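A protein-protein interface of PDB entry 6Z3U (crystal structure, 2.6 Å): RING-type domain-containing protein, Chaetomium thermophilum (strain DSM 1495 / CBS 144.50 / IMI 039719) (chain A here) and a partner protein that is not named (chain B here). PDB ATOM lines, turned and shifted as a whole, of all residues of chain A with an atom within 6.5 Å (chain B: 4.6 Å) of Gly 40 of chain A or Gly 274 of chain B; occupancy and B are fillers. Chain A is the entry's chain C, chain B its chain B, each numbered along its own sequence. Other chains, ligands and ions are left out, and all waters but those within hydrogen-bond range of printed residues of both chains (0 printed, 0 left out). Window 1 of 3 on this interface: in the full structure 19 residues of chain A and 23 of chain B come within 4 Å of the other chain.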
ATOM      1  N   GLN A  35      34.138 -28.566 -18.267  1.00  0.00           N
ATOM      2  CA  GLN A  35      33.785 -27.771 -17.096  1.00  0.00           C
ATOM      3  C   GLN A  35      32.440 -28.187 -16.514  1.00  0.00           C
ATOM      4  O   GLN A  35      32.246 -28.107 -15.296  1.00  0.00           O
ATOM      5  CB  GLN A  35      33.769 -26.286 -17.456  1.00  0.00           C
ATOM      6  CG  GLN A  35      34.737 -25.444 -16.635  1.00  0.00           C
ATOM      7  CD  GLN A  35      36.193 -25.796 -16.895  1.00  0.00           C
ATOM      8  OE1 GLN A  35      36.965 -26.018 -15.963  1.00  0.00           O
ATOM      9  NE2 GLN A  35      36.576 -25.837 -18.166  1.00  0.00           N
ATOM     10  N   HIS A  36      31.506 -28.637 -17.354  1.00  0.00           N
ATOM     11  CA  HIS A  36      30.191 -29.015 -16.848  1.00  0.00           C
ATOM     12  C   HIS A  36      30.244 -30.339 -16.099  1.00  0.00           C
ATOM     13  O   HIS A  36      29.622 -30.488 -15.043  1.00  0.00           O
ATOM     14  CB  HIS A  36      29.189 -29.106 -17.995  1.00  0.00           C
ATOM     15  CG  HIS A  36      28.691 -27.778 -18.467  1.00  0.00           C
ATOM     16  ND1 HIS A  36      29.498 -26.873 -19.121  1.00  0.00           N
ATOM     17  CD2 HIS A  36      27.469 -27.204 -18.385  1.00  0.00           C
ATOM     18  CE1 HIS A  36      28.792 -25.797 -19.421  1.00  0.00           C
ATOM     19  NE2 HIS A  36      27.559 -25.972 -18.983  1.00  0.00           N
ATOM     20  N   ILE A  37      30.980 -31.314 -16.630  1.00  0.00           N
ATOM     21  CA  ILE A  37      31.053 -32.618 -15.982  1.00  0.00           C
ATOM     22  C   ILE A  37      31.946 -32.555 -14.751  1.00  0.00           C
ATOM     23  O   ILE A  37      31.523 -32.901 -13.641  1.00  0.00           O
ATOM     24  CB  ILE A  37      31.529 -33.690 -16.985  1.00  0.00           C
ATOM     25  CG1 ILE A  37      32.898 -33.330 -17.574  1.00  0.00           C
ATOM     26  CG2 ILE A  37      30.493 -33.866 -18.088  1.00  0.00           C
ATOM     27  CD1 ILE A  37      33.224 -34.047 -18.872  1.00  0.00           C
ATOM     28  N   THR A  38      33.185 -32.090 -14.914  1.00  0.00           N
ATOM     29  CA  THR A  38      34.111 -32.051 -13.790  1.00  0.00           C
ATOM     30  C   THR A  38      33.667 -31.070 -12.710  1.00  0.00           C
ATOM     31  O   THR A  38      34.135 -31.170 -11.571  1.00  0.00           O
ATOM     32  CB  THR A  38      35.514 -31.687 -14.276  1.00  0.00           C
ATOM     33  OG1 THR A  38      36.488 -32.188 -13.352  1.00  0.00           O
ATOM     34  CG2 THR A  38      35.670 -30.180 -14.390  1.00  0.00           C
ATOM     35  N   GLY A  39      32.782 -30.130 -13.040  1.00  0.00           N
ATOM     36  CA  GLY A  39      32.282 -29.171 -12.076  1.00  0.00           C
ATOM     37  C   GLY A  39      31.017 -29.581 -11.362  1.00  0.00           C
ATOM     38  O   GLY A  39      30.630 -28.936 -10.382  1.00  0.00           O
ATOM     39  N   GLY A  40      30.358 -30.636 -11.831  1.00  0.00           N
ATOM     40  CA  GLY A  40      29.188 -31.153 -11.158  1.00  0.00           C
ATOM     41  C   GLY A  40      27.871 -30.561 -11.594  1.00  0.00           C
ATOM     42  O   GLY A  40      26.941 -30.493 -10.784  1.00  0.00           O
ATOM     43  N   TYR A  41      27.752 -30.133 -12.847  1.00  0.00           N
ATOM     44  CA  TYR A  41      26.469 -29.648 -13.336  1.00  0.00           C
ATOM     45  C   TYR A  41      25.531 -30.826 -13.564  1.00  0.00           C
ATOM     46  O   TYR A  41      25.905 -31.817 -14.199  1.00  0.00           O
ATOM     47  CB  TYR A  41      26.636 -28.855 -14.631  1.00  0.00           C
ATOM     48  CG  TYR A  41      25.333 -28.248 -15.107  1.00  0.00           C
ATOM     49  CD1 TYR A  41      24.439 -28.986 -15.874  1.00  0.00           C
ATOM     50  CD2 TYR A  41      24.988 -26.946 -14.774  1.00  0.00           C
ATOM     51  CE1 TYR A  41      23.244 -28.442 -16.302  1.00  0.00           C
ATOM     52  CE2 TYR A  41      23.794 -26.393 -15.197  1.00  0.00           C
ATOM     53  CZ  TYR A  41      22.926 -27.146 -15.959  1.00  0.00           C
ATOM     54  OH  TYR A  41      21.735 -26.605 -16.387  1.00  0.00           O
ATOM     55  N   SER A  42      24.313 -30.717 -13.044  1.00  0.00           N
ATOM     56  CA  SER A  42      23.324 -31.780 -13.139  1.00  0.00           C
ATOM     57  C   SER A  42      22.411 -31.511 -14.328  1.00  0.00           C
ATOM     58  O   SER A  42      21.612 -30.570 -14.307  1.00  0.00           O
ATOM     59  CB  SER A  42      22.509 -31.879 -11.852  1.00  0.00           C
ATOM     60  OG  SER A  42      21.430 -32.781 -12.017  1.00  0.00           O
ATOM     61  N   ASP A  45      18.669 -32.495 -13.365  1.00  0.00           N
ATOM     62  CA  ASP A  45      17.876 -31.446 -12.735  1.00  0.00           C
ATOM     63  C   ASP A  45      17.271 -30.510 -13.776  1.00  0.00           C
ATOM     64  O   ASP A  45      16.127 -30.066 -13.628  1.00  0.00           O
ATOM     65  CB  ASP A  45      18.740 -30.667 -11.743  1.00  0.00           C
ATOM     66  CG  ASP A  45      18.965 -31.422 -10.438  1.00  0.00           C
ATOM     67  OD1 ASP A  45      18.418 -32.536 -10.287  1.00  0.00           O
ATOM     68  OD2 ASP A  45      19.691 -30.902  -9.561  1.00  0.00           O
ATOM     69  N   LEU B 217      19.320 -22.753  -5.208  1.00  0.00           N
ATOM     70  CA  LEU B 217      20.537 -22.990  -4.446  1.00  0.00           C
ATOM     71  C   LEU B 217      20.651 -21.933  -3.355  1.00  0.00           C
ATOM     72  O   LEU B 217      20.440 -20.746  -3.616  1.00  0.00           O
ATOM     73  CB  LEU B 217      21.764 -22.948  -5.356  1.00  0.00           C
ATOM     74  CG  LEU B 217      21.845 -24.012  -6.451  1.00  0.00           C
ATOM     75  CD1 LEU B 217      23.015 -23.727  -7.384  1.00  0.00           C
ATOM     76  CD2 LEU B 217      21.975 -25.398  -5.842  1.00  0.00           C
ATOM     77  N   HIS B 272      30.056 -24.010 -13.455  1.00  0.00           N
ATOM     78  CA  HIS B 272      28.890 -24.808 -13.847  1.00  0.00           C
ATOM     79  C   HIS B 272      28.722 -25.921 -12.817  1.00  0.00           C
ATOM     80  O   HIS B 272      29.168 -27.052 -13.028  1.00  0.00           O
ATOM     81  CB  HIS B 272      29.060 -25.355 -15.263  1.00  0.00           C
ATOM     82  CG  HIS B 272      29.191 -24.292 -16.309  1.00  0.00           C
ATOM     83  ND1 HIS B 272      30.248 -24.245 -17.193  1.00  0.00           N
ATOM     84  CD2 HIS B 272      28.398 -23.239 -16.616  1.00  0.00           C
ATOM     85  CE1 HIS B 272      30.104 -23.205 -17.994  1.00  0.00           C
ATOM     86  NE2 HIS B 272      28.987 -22.580 -17.668  1.00  0.00           N
ATOM     87  N   TYR B 273      28.072 -25.597 -11.706  1.00  0.00           N
ATOM     88  CA  TYR B 273      27.867 -26.522 -10.601  1.00  0.00           C
ATOM     89  C   TYR B 273      26.374 -26.718 -10.350  1.00  0.00           C
ATOM     90  O   TYR B 273      25.524 -26.166 -11.051  1.00  0.00           O
ATOM     91  CB  TYR B 273      28.571 -26.014  -9.339  1.00  0.00           C
ATOM     92  CG  TYR B 273      28.235 -24.584  -8.965  1.00  0.00           C
ATOM     93  CD1 TYR B 273      27.112 -24.291  -8.203  1.00  0.00           C
ATOM     94  CD2 TYR B 273      29.047 -23.530  -9.363  1.00  0.00           C
ATOM     95  CE1 TYR B 273      26.805 -22.987  -7.852  1.00  0.00           C
ATOM     96  CE2 TYR B 273      28.748 -22.223  -9.019  1.00  0.00           C
ATOM     97  CZ  TYR B 273      27.626 -21.959  -8.263  1.00  0.00           C
ATOM     98  OH  TYR B 273      27.331 -20.660  -7.920  1.00  0.00           O
ATOM     99  N   GLY B 274      26.061 -27.519  -9.334  1.00  0.00           N
ATOM    100  CA  GLY B 274      24.684 -27.841  -9.015  1.00  0.00           C
ATOM    101  C   GLY B 274      24.419 -27.950  -7.528  1.00  0.00           C
ATOM    102  O   GLY B 274      25.128 -27.350  -6.716  1.00  0.00           O
ATOM    103  N   GLY B 275      23.394 -28.723  -7.158  1.00  0.00           N
ATOM    104  CA  GLY B 275      23.013 -28.823  -5.759  1.00  0.00           C
ATOM    105  C   GLY B 275      24.116 -29.354  -4.868  1.00  0.00           C
ATOM    106  O   GLY B 275      24.133 -29.080  -3.665  1.00  0.00           O
ATOM    107  N   ALA B 276      25.048 -30.122  -5.437  1.00  0.00           N
ATOM    108  CA  ALA B 276      26.094 -30.731  -4.623  1.00  0.00           C
ATOM    109  C   ALA B 276      26.847 -29.694  -3.801  1.00  0.00           C
ATOM    110  O   ALA B 276      27.370 -30.014  -2.727  1.00  0.00           O
ATOM    111  CB  ALA B 276      27.065 -31.507  -5.515  1.00  0.00           C
ATOM    112  N   VAL B 277      26.907 -28.448  -4.274  1.00  0.00           N
ATOM    113  CA  VAL B 277      27.639 -27.424  -3.536  1.00  0.00           C
ATOM    114  C   VAL B 277      26.993 -27.180  -2.178  1.00  0.00           C
ATOM    115  O   VAL B 277      27.685 -26.915  -1.188  1.00  0.00           O
ATOM    116  CB  VAL B 277      27.730 -26.124  -4.356  1.00  0.00           C
ATOM    117  CG1 VAL B 277      28.549 -26.351  -5.613  1.00  0.00           C
ATOM    118  CG2 VAL B 277      26.342 -25.592  -4.689  1.00  0.00           C
ATOM    119  N   PRO B 368      31.809 -33.643  -6.950  1.00  0.00           N
ATOM    120  CA  PRO B 368      30.382 -33.408  -6.666  1.00  0.00           C
ATOM    121  C   PRO B 368      29.456 -34.382  -7.366  1.00  0.00           C
ATOM    122  O   PRO B 368      28.307 -34.538  -6.935  1.00  0.00           O
ATOM    123  CB  PRO B 368      30.154 -31.968  -7.150  1.00  0.00           C
ATOM    124  CG  PRO B 368      31.255 -31.701  -8.112  1.00  0.00           C
ATOM    125  CD  PRO B 368      32.432 -32.495  -7.635  1.00  0.00           C
ATOM    126  N   LYS B 369      29.914 -35.038  -8.434  1.00  0.00           N
ATOM    127  CA  LYS B 369      29.062 -35.987  -9.140  1.00  0.00           C
ATOM    128  C   LYS B 369      28.748 -37.209  -8.286  1.00  0.00           C
ATOM    129  O   LYS B 369      27.638 -37.749  -8.366  1.00  0.00           O
ATOM    130  CB  LYS B 369      29.732 -36.401 -10.450  1.00  0.00           C
ATOM    131  CG  LYS B 369      29.918 -35.250 -11.431  1.00  0.00           C
ATOM    132  CD  LYS B 369      30.694 -35.677 -12.665  1.00  0.00           C
ATOM    133  CE  LYS B 369      32.185 -35.810 -12.379  1.00  0.00           C
ATOM    134  NZ  LYS B 369      32.944 -36.400 -13.528  1.00  0.00           N
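The backbone NH of Tyr 41 of chain A lies within hydrogen-bond range of the backbone carbonyl oxygen of His 36 of chain A, at 2.9 Å.
Among the printed residues, merely in contact across the chains: Ile 37 of chain A with Lys 369 of chain B (3.1 Å), Gly 39 of chain A with His 272 of chain B (3.5 Å), Gly 39 of chain A with Pro 368 of chain B (3.6 Å), Gly 39 of chain A with Tyr 273 of chain B (3.7 Å), Gly 40 of chain A with Pro 368 of chain B (3.7 Å), Tyr 41 of chain A with Tyr 273 of chain B (3.8 Å), Gly 40 of chain A with Tyr 273 of chain B (3.8 Å), Gly 40 of chain A with His 272 of chain B (3.96 Å) and Gln 35 of chain A with His 272 of chain B (3.97 Å).
Hydrophobic or aromatic side chains of chain A within 4 Å of the printed part of chain B: His 36 and Tyr 41. Along chain A the printed residues that touch a printed residue of chain B span positions 35 to 41. Printed residues of chain B that touch a printed residue of chain A: His 272, Tyr 273, Gly 274, Pro 368 and Lys 369.
Printed residues of chain B within 4 Å of Ile 37 of chain A: Lys 369 (3.1 Å). Of the printed residues of chain B, Gly 39 of chain A touches His 272, Tyr 273 and Pro 368. Of the printed residues of chain B, Tyr 41 of chain A touches His 272 (3.4 Å) and Tyr 273 (3.8 Å). Gly 274 of chain B touches one residue of chain A. Printed residues of chain A within 4 Å of Pro 368 of chain B: Gly 39 and Gly 40. The nearest residue of chain B that does not touch Gly 40 of chain A is Lys 369 of chain B (4.2 Å). The nearest printed residue of chain A that does not touch Tyr 273 of chain B is Ser 42 of chain A (5.1 Å).
N of Gly 274 of chain B sits at hydrogen-bond distance from O of Gly 40 of chain A (3.4 Å). The backbone carbonyl oxygen of His 272 of chain B is in hydrogen-bond range of the backbone NH of Tyr 41 of chain A (3.4 Å). A ring nitrogen (ND1) of His 36 of chain A sits close to a ring nitrogen (ND1) of His 272 of chain B (3.3 Å).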
